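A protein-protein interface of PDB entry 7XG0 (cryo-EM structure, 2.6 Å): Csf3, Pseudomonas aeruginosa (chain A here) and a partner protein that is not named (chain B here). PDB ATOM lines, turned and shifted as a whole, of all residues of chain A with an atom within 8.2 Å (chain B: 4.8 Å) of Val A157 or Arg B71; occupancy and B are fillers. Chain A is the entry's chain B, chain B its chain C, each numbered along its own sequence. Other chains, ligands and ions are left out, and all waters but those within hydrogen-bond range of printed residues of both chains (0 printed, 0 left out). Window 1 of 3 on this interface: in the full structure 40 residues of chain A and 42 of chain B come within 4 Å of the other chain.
O of Gly A156 lies within hydrogen-bond range of N of Val B146 (3.1 Å). OD1 of Asp B147 lies within hydrogen-bond range of ND2 of Asn A12, 3.4 Å away. The backbone carbonyl oxygen (O) of Gly A158 lies close to the side-chain carboxylate (OD1) of Asp B147 (2.9 Å). The backbone carbonyl oxygen (O) of Gly A156 lies within hydrogen-bond range of the guanidinium group (NH1) of Arg B71 (2.7 Å). The backbone carbonyl oxygen (O) of Val B146 sits at hydrogen-bond distance from the backbone NH (N) of Gly A158, 3.2 Å away. The side-chain amide nitrogen of Asn B68 sits close to the side-chain amide nitrogen of Gln A84 (3.5 Å). The side-chain carboxylate (OD2) of Asp B147 sits at hydrogen-bond distance from the side-chain amide nitrogen (NE2) of Gln A161, 2.4 Å away. O of Val B146 lies close to O of Val A157 (3.3 Å).
The backbone carbonyl oxygen of Leu B132 lies within hydrogen-bond range of the backbone NH of Leu B144, at 3.2 Å. The backbone NH (N) of Gly B67 is in hydrogen-bond range of the side-chain hydroxyl (OG) of Ser B148, at 3.3 Å. NH1 of Arg B71 is in hydrogen-bond range of O of Leu B144, at 2.5 Å. ND2 of Asn A12 is in hydrogen-bond range of O of Gly A158 (3.1 Å). The backbone carbonyl oxygen of Arg A155 lies close to the side-chain amide oxygen of Gln A150 (3.0 Å). O of Gly A158 lies close to OE1 of Gln A161, at 3.1 Å.
Among the printed residues, pairs that only touch across the chains: Tyr A121 with Asn B68 (3.9 Å), Gln A150 with Met B145 (3.5 Å), Arg A155 with Met B145 (3.2 Å), Gly A156 with Leu B144 (3.8 Å), Gly A156 with Met B145 (3.7 Å), Val A157 with Gly B67 (3.7 Å), Val A157 with Asn B68 (3.7 Å), Val A157 with Arg B71 (3.9 Å) and Gly A158 with Met B145 (3.8 Å).
Met A15 touches none of the printed residues of chain B. Printed residues of chain B within 4 Å of Arg A155: Met B145 (3.2 Å). Of the printed residues of chain B, Gly A156 touches Arg B71, Leu B144, Met B145 and Val B146. Val A157 touches just these residues of chain B: Gly B67 (3.7 Å), Asn B68 (3.7 Å), Arg B71 (3.9 Å) and Val B146 (3.0 Å). Printed residues of chain B within 4 Å of Gly A158: Met B145 (3.8 Å), Val B146 (3.2 Å) and Asp B147 (2.9 Å). Gly A160 touches none of the printed residues of chain B. Arg B71 touches just these residues of chain A: Gly A156 (2.7 Å) and Val A157 (3.9 Å). Of the printed residues of chain A, Val B146 touches Gly A156, Val A157 and Gly A158. The nearest printed residue of chain B that does not touch Val A157 is Ser B148 (4.6 Å). The nearest residue of chain A that does not touch Arg B71 is Arg A155 (5.7 Å).
Of the 17 printed residues of chain B, 7 touch a printed residue of chain A. Hydrophobic or aromatic side chains of chain B that line the printed part of chain A: Met B145. Among the printed residues, 17 pairs touch across the chains.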
ATOM      1  N   ASN A  12     -16.157  -0.476 -11.140  1.00  0.00           N
ATOM      2  CA  ASN A  12     -17.556  -0.303 -10.790  1.00  0.00           C
ATOM      3  C   ASN A  12     -18.122  -1.632 -10.292  1.00  0.00           C
ATOM      4  O   ASN A  12     -17.626  -2.699 -10.667  1.00  0.00           O
ATOM      5  CB  ASN A  12     -18.388   0.194 -11.976  1.00  0.00           C
ATOM      6  CG  ASN A  12     -17.667   1.196 -12.852  1.00  0.00           C
ATOM      7  OD1 ASN A  12     -16.775   1.919 -12.415  1.00  0.00           O
ATOM      8  ND2 ASN A  12     -18.123   1.301 -14.089  1.00  0.00           N
ATOM      9  N   MET A  15     -23.196  -5.789 -12.422  1.00  0.00           N
ATOM     10  CA  MET A  15     -24.572  -6.244 -12.526  1.00  0.00           C
ATOM     11  C   MET A  15     -24.652  -7.706 -12.127  1.00  0.00           C
ATOM     12  O   MET A  15     -24.084  -8.571 -12.802  1.00  0.00           O
ATOM     13  CB  MET A  15     -25.070  -6.059 -13.958  1.00  0.00           C
ATOM     14  CG  MET A  15     -25.533  -4.652 -14.308  1.00  0.00           C
ATOM     15  SD  MET A  15     -27.124  -4.066 -13.689  1.00  0.00           S
ATOM     16  CE  MET A  15     -28.024  -5.569 -13.419  1.00  0.00           C
ATOM     17  N   TRP A  82     -30.246  -1.582  -8.346  1.00  0.00           N
ATOM     18  CA  TRP A  82     -30.239  -0.517  -9.337  1.00  0.00           C
ATOM     19  C   TRP A  82     -31.620  -0.435  -9.968  1.00  0.00           C
ATOM     20  O   TRP A  82     -32.128  -1.433 -10.491  1.00  0.00           O
ATOM     21  CB  TRP A  82     -29.186  -0.783 -10.412  1.00  0.00           C
ATOM     22  CG  TRP A  82     -28.744   0.433 -11.153  1.00  0.00           C
ATOM     23  CD1 TRP A  82     -28.924   0.694 -12.477  1.00  0.00           C
ATOM     24  CD2 TRP A  82     -28.011   1.540 -10.620  1.00  0.00           C
ATOM     25  NE1 TRP A  82     -28.370   1.910 -12.799  1.00  0.00           N
ATOM     26  CE2 TRP A  82     -27.803   2.449 -11.675  1.00  0.00           C
ATOM     27  CE3 TRP A  82     -27.524   1.860  -9.349  1.00  0.00           C
ATOM     28  CZ2 TRP A  82     -27.121   3.649 -11.499  1.00  0.00           C
ATOM     29  CZ3 TRP A  82     -26.853   3.052  -9.177  1.00  0.00           C
ATOM     30  CH2 TRP A  82     -26.658   3.933 -10.245  1.00  0.00           C
ATOM     31  N   GLN A  84     -33.646   1.044 -13.080  1.00  0.00           N
ATOM     32  CA  GLN A  84     -33.562   1.691 -14.375  1.00  0.00           C
ATOM     33  C   GLN A  84     -34.964   1.752 -14.954  1.00  0.00           C
ATOM     34  O   GLN A  84     -35.849   0.991 -14.549  1.00  0.00           O
ATOM     35  CB  GLN A  84     -32.593   0.969 -15.314  1.00  0.00           C
ATOM     36  CG  GLN A  84     -31.140   1.391 -15.148  1.00  0.00           C
ATOM     37  CD  GLN A  84     -30.201   0.680 -16.105  1.00  0.00           C
ATOM     38  OE1 GLN A  84     -29.003   0.959 -16.139  1.00  0.00           O
ATOM     39  NE2 GLN A  84     -30.742  -0.249 -16.886  1.00  0.00           N
ATOM     40  N   TYR A 121     -37.648  -1.169 -13.713  1.00  0.00           N
ATOM     41  CA  TYR A 121     -37.110  -2.489 -13.426  1.00  0.00           C
ATOM     42  C   TYR A 121     -35.902  -2.349 -12.513  1.00  0.00           C
ATOM     43  O   TYR A 121     -35.014  -1.523 -12.752  1.00  0.00           O
ATOM     44  CB  TYR A 121     -36.752  -3.268 -14.711  1.00  0.00           C
ATOM     45  CG  TYR A 121     -35.690  -2.666 -15.607  1.00  0.00           C
ATOM     46  CD1 TYR A 121     -35.965  -1.573 -16.423  1.00  0.00           C
ATOM     47  CD2 TYR A 121     -34.422  -3.228 -15.672  1.00  0.00           C
ATOM     48  CE1 TYR A 121     -34.996  -1.031 -17.238  1.00  0.00           C
ATOM     49  CE2 TYR A 121     -33.448  -2.701 -16.497  1.00  0.00           C
ATOM     50  CZ  TYR A 121     -33.745  -1.610 -17.284  1.00  0.00           C
ATOM     51  OH  TYR A 121     -32.778  -1.074 -18.100  1.00  0.00           O
ATOM     52  N   ILE A 125     -27.006  -5.283  -7.759  1.00  0.00           N
ATOM     53  CA  ILE A 125     -25.696  -4.711  -8.046  1.00  0.00           C
ATOM     54  C   ILE A 125     -24.748  -5.147  -6.935  1.00  0.00           C
ATOM     55  O   ILE A 125     -25.057  -4.975  -5.747  1.00  0.00           O
ATOM     56  CB  ILE A 125     -25.777  -3.175  -8.145  1.00  0.00           C
ATOM     57  CG1 ILE A 125     -26.273  -2.751  -9.522  1.00  0.00           C
ATOM     58  CG2 ILE A 125     -24.435  -2.525  -7.918  1.00  0.00           C
ATOM     59  CD1 ILE A 125     -25.369  -3.155 -10.638  1.00  0.00           C
ATOM     60  N   GLN A 150     -15.069  -5.190 -19.697  1.00  0.00           N
ATOM     61  CA  GLN A 150     -16.114  -5.266 -18.685  1.00  0.00           C
ATOM     62  C   GLN A 150     -16.586  -6.704 -18.557  1.00  0.00           C
ATOM     63  O   GLN A 150     -16.439  -7.509 -19.479  1.00  0.00           O
ATOM     64  CB  GLN A 150     -17.342  -4.387 -18.977  1.00  0.00           C
ATOM     65  CG  GLN A 150     -17.097  -3.054 -19.647  1.00  0.00           C
ATOM     66  CD  GLN A 150     -18.306  -2.611 -20.437  1.00  0.00           C
ATOM     67  OE1 GLN A 150     -19.343  -2.275 -19.863  1.00  0.00           O
ATOM     68  NE2 GLN A 150     -18.208  -2.665 -21.759  1.00  0.00           N
ATOM     69  N   GLY A 153     -23.596  -8.377 -16.789  1.00  0.00           N
ATOM     70  CA  GLY A 153     -24.644  -7.908 -17.670  1.00  0.00           C
ATOM     71  C   GLY A 153     -24.725  -6.395 -17.739  1.00  0.00           C
ATOM     72  O   GLY A 153     -23.976  -5.708 -17.045  1.00  0.00           O
ATOM     73  N   LYS A 154     -25.651  -5.926 -18.585  1.00  0.00           N
ATOM     74  CA  LYS A 154     -25.923  -4.502 -18.839  1.00  0.00           C
ATOM     75  C   LYS A 154     -24.645  -3.727 -19.149  1.00  0.00           C
ATOM     76  O   LYS A 154     -24.343  -2.698 -18.541  1.00  0.00           O
ATOM     77  CB  LYS A 154     -26.689  -3.870 -17.676  1.00  0.00           C
ATOM     78  CG  LYS A 154     -28.162  -3.608 -17.971  1.00  0.00           C
ATOM     79  CD  LYS A 154     -28.950  -4.894 -18.154  1.00  0.00           C
ATOM     80  CE  LYS A 154     -30.415  -4.602 -18.455  1.00  0.00           C
ATOM     81  NZ  LYS A 154     -30.572  -3.675 -19.611  1.00  0.00           N
ATOM     82  N   ARG A 155     -23.864  -4.261 -20.085  1.00  0.00           N
ATOM     83  CA  ARG A 155     -22.588  -3.644 -20.414  1.00  0.00           C
ATOM     84  C   ARG A 155     -22.755  -2.384 -21.247  1.00  0.00           C
ATOM     85  O   ARG A 155     -21.830  -1.573 -21.304  1.00  0.00           O
ATOM     86  CB  ARG A 155     -21.700  -4.643 -21.143  1.00  0.00           C
ATOM     87  CG  ARG A 155     -21.049  -5.646 -20.217  1.00  0.00           C
ATOM     88  CD  ARG A 155     -20.262  -6.660 -21.006  1.00  0.00           C
ATOM     89  NE  ARG A 155     -20.936  -6.996 -22.253  1.00  0.00           N
ATOM     90  CZ  ARG A 155     -21.832  -7.964 -22.388  1.00  0.00           C
ATOM     91  NH1 ARG A 155     -22.198  -8.712 -21.361  1.00  0.00           N
ATOM     92  NH2 ARG A 155     -22.380  -8.180 -23.579  1.00  0.00           N
ATOM     93  N   GLY A 156     -23.909  -2.201 -21.888  1.00  0.00           N
ATOM     94  CA  GLY A 156     -24.167  -0.979 -22.625  1.00  0.00           C
ATOM     95  C   GLY A 156     -24.335   0.250 -21.759  1.00  0.00           C
ATOM     96  O   GLY A 156     -24.156   1.366 -22.259  1.00  0.00           O
ATOM     97  N   VAL A 157     -24.660   0.076 -20.478  1.00  0.00           N
ATOM     98  CA  VAL A 157     -24.809   1.204 -19.567  1.00  0.00           C
ATOM     99  C   VAL A 157     -23.630   1.224 -18.602  1.00  0.00           C
ATOM    100  O   VAL A 157     -23.730   1.738 -17.482  1.00  0.00           O
ATOM    101  CB  VAL A 157     -26.163   1.160 -18.834  1.00  0.00           C
ATOM    102  CG1 VAL A 157     -27.287   1.374 -19.827  1.00  0.00           C
ATOM    103  CG2 VAL A 157     -26.356  -0.156 -18.115  1.00  0.00           C
ATOM    104  N   GLY A 158     -22.496   0.684 -19.049  1.00  0.00           N
ATOM    105  CA  GLY A 158     -21.212   0.932 -18.424  1.00  0.00           C
ATOM    106  C   GLY A 158     -20.971   0.247 -17.100  1.00  0.00           C
ATOM    107  O   GLY A 158     -20.086   0.678 -16.353  1.00  0.00           O
ATOM    108  N   PHE A 159     -21.713  -0.807 -16.787  1.00  0.00           N
ATOM    109  CA  PHE A 159     -21.599  -1.465 -15.496  1.00  0.00           C
ATOM    110  C   PHE A 159     -20.452  -2.462 -15.466  1.00  0.00           C
ATOM    111  O   PHE A 159     -20.322  -3.323 -16.340  1.00  0.00           O
ATOM    112  CB  PHE A 159     -22.895  -2.185 -15.141  1.00  0.00           C
ATOM    113  CG  PHE A 159     -23.830  -1.359 -14.328  1.00  0.00           C
ATOM    114  CD1 PHE A 159     -23.450  -0.911 -13.074  1.00  0.00           C
ATOM    115  CD2 PHE A 159     -25.081  -1.021 -14.812  1.00  0.00           C
ATOM    116  CE1 PHE A 159     -24.302  -0.142 -12.315  1.00  0.00           C
ATOM    117  CE2 PHE A 159     -25.940  -0.253 -14.058  1.00  0.00           C
ATOM    118  CZ  PHE A 159     -25.547   0.183 -12.806  1.00  0.00           C
ATOM    119  N   GLY A 160     -19.632  -2.346 -14.426  1.00  0.00           N
ATOM    120  CA  GLY A 160     -18.681  -3.385 -14.105  1.00  0.00           C
ATOM    121  C   GLY A 160     -17.496  -3.524 -15.027  1.00  0.00           C
ATOM    122  O   GLY A 160     -17.188  -4.646 -15.443  1.00  0.00           O
ATOM    123  N   GLN A 161     -16.835  -2.427 -15.394  1.00  0.00           N
ATOM    124  CA  GLN A 161     -15.622  -2.571 -16.186  1.00  0.00           C
ATOM    125  C   GLN A 161     -14.484  -3.117 -15.333  1.00  0.00           C
ATOM    126  O   GLN A 161     -14.344  -2.768 -14.158  1.00  0.00           O
ATOM    127  CB  GLN A 161     -15.206  -1.258 -16.857  1.00  0.00           C
ATOM    128  CG  GLN A 161     -15.114  -0.042 -15.984  1.00  0.00           C
ATOM    129  CD  GLN A 161     -16.094   1.024 -16.408  1.00  0.00           C
ATOM    130  OE1 GLN A 161     -17.094   0.724 -17.069  1.00  0.00           O
ATOM    131  NE2 GLN A 161     -15.843   2.262 -16.012  1.00  0.00           N
ATOM    132  N   GLY B  67     -25.647   5.320 -15.993  1.00  0.00           N
ATOM    133  CA  GLY B  67     -25.241   5.135 -17.374  1.00  0.00           C
ATOM    134  C   GLY B  67     -26.416   4.988 -18.320  1.00  0.00           C
ATOM    135  O   GLY B  67     -26.293   5.269 -19.512  1.00  0.00           O
ATOM    136  N   ASN B  68     -27.565   4.544 -17.802  1.00  0.00           N
ATOM    137  CA  ASN B  68     -28.792   4.534 -18.592  1.00  0.00           C
ATOM    138  C   ASN B  68     -29.250   5.950 -18.917  1.00  0.00           C
ATOM    139  O   ASN B  68     -29.643   6.239 -20.056  1.00  0.00           O
ATOM    140  CB  ASN B  68     -29.881   3.781 -17.832  1.00  0.00           C
ATOM    141  CG  ASN B  68     -30.862   3.093 -18.750  1.00  0.00           C
ATOM    142  OD1 ASN B  68     -30.599   2.908 -19.937  1.00  0.00           O
ATOM    143  ND2 ASN B  68     -32.013   2.724 -18.205  1.00  0.00           N
ATOM    144  N   THR B  69     -29.193   6.847 -17.925  1.00  0.00           N
ATOM    145  CA  THR B  69     -29.594   8.236 -18.127  1.00  0.00           C
ATOM    146  C   THR B  69     -28.659   8.948 -19.097  1.00  0.00           C
ATOM    147  O   THR B  69     -29.117   9.639 -20.013  1.00  0.00           O
ATOM    148  CB  THR B  69     -29.639   8.965 -16.782  1.00  0.00           C
ATOM    149  OG1 THR B  69     -30.657   8.384 -15.958  1.00  0.00           O
ATOM    150  CG2 THR B  69     -29.951  10.442 -16.970  1.00  0.00           C
ATOM    151  N   MET B  70     -27.346   8.753 -18.939  1.00  0.00           N
ATOM    152  CA  MET B  70     -26.387   9.336 -19.874  1.00  0.00           C
ATOM    153  C   MET B  70     -26.477   8.713 -21.261  1.00  0.00           C
ATOM    154  O   MET B  70     -26.281   9.413 -22.259  1.00  0.00           O
ATOM    155  CB  MET B  70     -24.967   9.204 -19.330  1.00  0.00           C
ATOM    156  CG  MET B  70     -24.705  10.029 -18.098  1.00  0.00           C
ATOM    157  SD  MET B  70     -25.315  11.699 -18.373  1.00  0.00           S
ATOM    158  CE  MET B  70     -23.781  12.548 -18.714  1.00  0.00           C
ATOM    159  N   ARG B  71     -26.781   7.415 -21.342  1.00  0.00           N
ATOM    160  CA  ARG B  71     -26.909   6.749 -22.634  1.00  0.00           C
ATOM    161  C   ARG B  71     -28.117   7.273 -23.401  1.00  0.00           C
ATOM    162  O   ARG B  71     -28.021   7.589 -24.594  1.00  0.00           O
ATOM    163  CB  ARG B  71     -27.004   5.238 -22.424  1.00  0.00           C
ATOM    164  CG  ARG B  71     -27.065   4.421 -23.699  1.00  0.00           C
ATOM    165  CD  ARG B  71     -27.062   2.937 -23.381  1.00  0.00           C
ATOM    166  NE  ARG B  71     -27.198   2.120 -24.581  1.00  0.00           N
ATOM    167  CZ  ARG B  71     -26.184   1.547 -25.215  1.00  0.00           C
ATOM    168  NH1 ARG B  71     -24.939   1.684 -24.791  1.00  0.00           N
ATOM    169  NH2 ARG B  71     -26.426   0.819 -26.301  1.00  0.00           N
ATOM    170  N   SER B  72     -29.254   7.418 -22.719  1.00  0.00           N
ATOM    171  CA  SER B  72     -30.424   7.976 -23.381  1.00  0.00           C
ATOM    172  C   SER B  72     -30.284   9.473 -23.619  1.00  0.00           C
ATOM    173  O   SER B  72     -30.868   9.994 -24.568  1.00  0.00           O
ATOM    174  CB  SER B  72     -31.683   7.690 -22.576  1.00  0.00           C
ATOM    175  OG  SER B  72     -32.846   7.980 -23.332  1.00  0.00           O
ATOM    176  N   LEU B  73     -29.513  10.177 -22.783  1.00  0.00           N
ATOM    177  CA  LEU B  73     -29.241  11.588 -23.038  1.00  0.00           C
ATOM    178  C   LEU B  73     -28.396  11.767 -24.290  1.00  0.00           C
ATOM    179  O   LEU B  73     -28.674  12.650 -25.110  1.00  0.00           O
ATOM    180  CB  LEU B  73     -28.549  12.214 -21.828  1.00  0.00           C
ATOM    181  CG  LEU B  73     -28.048  13.646 -22.020  1.00  0.00           C
ATOM    182  CD1 LEU B  73     -29.207  14.609 -22.221  1.00  0.00           C
ATOM    183  CD2 LEU B  73     -27.185  14.070 -20.850  1.00  0.00           C
ATOM    184  N   LEU B  74     -27.375  10.923 -24.459  1.00  0.00           N
ATOM    185  CA  LEU B  74     -26.568  10.936 -25.674  1.00  0.00           C
ATOM    186  C   LEU B  74     -27.401  10.546 -26.891  1.00  0.00           C
ATOM    187  O   LEU B  74     -27.251  11.136 -27.968  1.00  0.00           O
ATOM    188  CB  LEU B  74     -25.377   9.994 -25.506  1.00  0.00           C
ATOM    189  CG  LEU B  74     -24.213  10.095 -26.488  1.00  0.00           C
ATOM    190  CD1 LEU B  74     -23.564  11.467 -26.426  1.00  0.00           C
ATOM    191  CD2 LEU B  74     -23.195   9.005 -26.204  1.00  0.00           C
ATOM    192  N   ARG B  75     -28.306   9.573 -26.724  1.00  0.00           N
ATOM    193  CA  ARG B  75     -29.199   9.160 -27.806  1.00  0.00           C
ATOM    194  C   ARG B  75     -30.143  10.285 -28.218  1.00  0.00           C
ATOM    195  O   ARG B  75     -30.318  10.557 -29.412  1.00  0.00           O
ATOM    196  CB  ARG B  75     -29.994   7.930 -27.368  1.00  0.00           C
ATOM    197  CG  ARG B  75     -31.001   7.437 -28.388  1.00  0.00           C
ATOM    198  CD  ARG B  75     -32.151   6.713 -27.711  1.00  0.00           C
ATOM    199  NE  ARG B  75     -31.722   5.494 -27.035  1.00  0.00           N
ATOM    200  CZ  ARG B  75     -31.660   4.300 -27.609  1.00  0.00           C
ATOM    201  NH1 ARG B  75     -31.991   4.126 -28.877  1.00  0.00           N
ATOM    202  NH2 ARG B  75     -31.259   3.255 -26.891  1.00  0.00           N
ATOM    203  N   LEU B 132     -24.937   2.129 -32.947  1.00  0.00           N
ATOM    204  CA  LEU B 132     -24.516   2.634 -31.644  1.00  0.00           C
ATOM    205  C   LEU B 132     -25.357   2.042 -30.519  1.00  0.00           C
ATOM    206  O   LEU B 132     -24.820   1.595 -29.500  1.00  0.00           O
ATOM    207  CB  LEU B 132     -24.590   4.160 -31.622  1.00  0.00           C
ATOM    208  CG  LEU B 132     -23.557   4.863 -32.498  1.00  0.00           C
ATOM    209  CD1 LEU B 132     -23.730   6.363 -32.437  1.00  0.00           C
ATOM    210  CD2 LEU B 132     -22.165   4.475 -32.062  1.00  0.00           C
ATOM    211  N   PHE B 133     -26.675   2.020 -30.684  1.00  0.00           N
ATOM    212  CA  PHE B 133     -27.546   1.618 -29.590  1.00  0.00           C
ATOM    213  C   PHE B 133     -28.228   0.279 -29.820  1.00  0.00           C
ATOM    214  O   PHE B 133     -28.352  -0.504 -28.873  1.00  0.00           O
ATOM    215  CB  PHE B 133     -28.591   2.706 -29.333  1.00  0.00           C
ATOM    216  CG  PHE B 133     -27.987   4.021 -28.934  1.00  0.00           C
ATOM    217  CD1 PHE B 133     -27.606   4.251 -27.621  1.00  0.00           C
ATOM    218  CD2 PHE B 133     -27.772   5.015 -29.877  1.00  0.00           C
ATOM    219  CE1 PHE B 133     -27.033   5.454 -27.252  1.00  0.00           C
ATOM    220  CE2 PHE B 133     -27.201   6.220 -29.515  1.00  0.00           C
ATOM    221  CZ  PHE B 133     -26.827   6.438 -28.201  1.00  0.00           C
ATOM    222  N   GLY B 142     -25.539  -2.837 -29.354  1.00  0.00           N
ATOM    223  CA  GLY B 142     -24.903  -1.655 -29.883  1.00  0.00           C
ATOM    224  C   GLY B 142     -23.397  -1.667 -29.715  1.00  0.00           C
ATOM    225  O   GLY B 142     -22.830  -2.416 -28.919  1.00  0.00           O
ATOM    226  N   LEU B 144     -21.839   0.886 -28.564  1.00  0.00           N
ATOM    227  CA  LEU B 144     -21.565   1.946 -27.607  1.00  0.00           C
ATOM    228  C   LEU B 144     -21.748   1.443 -26.182  1.00  0.00           C
ATOM    229  O   LEU B 144     -22.813   0.922 -25.833  1.00  0.00           O
ATOM    230  CB  LEU B 144     -22.493   3.134 -27.863  1.00  0.00           C
ATOM    231  CG  LEU B 144     -22.093   4.550 -27.473  1.00  0.00           C
ATOM    232  CD1 LEU B 144     -21.124   5.085 -28.491  1.00  0.00           C
ATOM    233  CD2 LEU B 144     -23.330   5.422 -27.428  1.00  0.00           C
ATOM    234  N   MET B 145     -20.709   1.597 -25.365  1.00  0.00           N
ATOM    235  CA  MET B 145     -20.815   1.498 -23.918  1.00  0.00           C
ATOM    236  C   MET B 145     -20.778   2.918 -23.381  1.00  0.00           C
ATOM    237  O   MET B 145     -19.892   3.697 -23.747  1.00  0.00           O
ATOM    238  CB  MET B 145     -19.686   0.647 -23.329  1.00  0.00           C
ATOM    239  CG  MET B 145     -19.564   0.663 -21.799  1.00  0.00           C
ATOM    240  SD  MET B 145     -17.960   1.095 -21.079  1.00  0.00           S
ATOM    241  CE  MET B 145     -17.875   2.863 -21.313  1.00  0.00           C
ATOM    242  N   VAL B 146     -21.758   3.269 -22.559  1.00  0.00           N
ATOM    243  CA  VAL B 146     -21.836   4.589 -21.950  1.00  0.00           C
ATOM    244  C   VAL B 146     -21.695   4.394 -20.449  1.00  0.00           C
ATOM    245  O   VAL B 146     -22.550   3.763 -19.818  1.00  0.00           O
ATOM    246  CB  VAL B 146     -23.150   5.302 -22.311  1.00  0.00           C
ATOM    247  CG1 VAL B 146     -23.435   6.448 -21.358  1.00  0.00           C
ATOM    248  CG2 VAL B 146     -23.096   5.810 -23.735  1.00  0.00           C
ATOM    249  N   ASP B 147     -20.613   4.907 -19.880  1.00  0.00           N
ATOM    250  CA  ASP B 147     -20.430   4.761 -18.448  1.00  0.00           C
ATOM    251  C   ASP B 147     -21.327   5.745 -17.704  1.00  0.00           C
ATOM    252  O   ASP B 147     -21.941   6.642 -18.288  1.00  0.00           O
ATOM    253  CB  ASP B 147     -18.966   4.973 -18.061  1.00  0.00           C
ATOM    254  CG  ASP B 147     -18.551   4.140 -16.867  1.00  0.00           C
ATOM    255  OD1 ASP B 147     -19.435   3.543 -16.221  1.00  0.00           O
ATOM    256  OD2 ASP B 147     -17.337   4.083 -16.578  1.00  0.00           O
ATOM    257  N   SER B 148     -21.419   5.544 -16.396  1.00  0.00           N
ATOM    258  CA  SER B 148     -22.064   6.514 -15.534  1.00  0.00           C
ATOM    259  C   SER B 148     -21.249   7.805 -15.502  1.00  0.00           C
ATOM    260  O   SER B 148     -20.033   7.807 -15.704  1.00  0.00           O
ATOM    261  CB  SER B 148     -22.220   5.944 -14.127  1.00  0.00           C
ATOM    262  OG  SER B 148     -22.970   4.741 -14.144  1.00  0.00           O
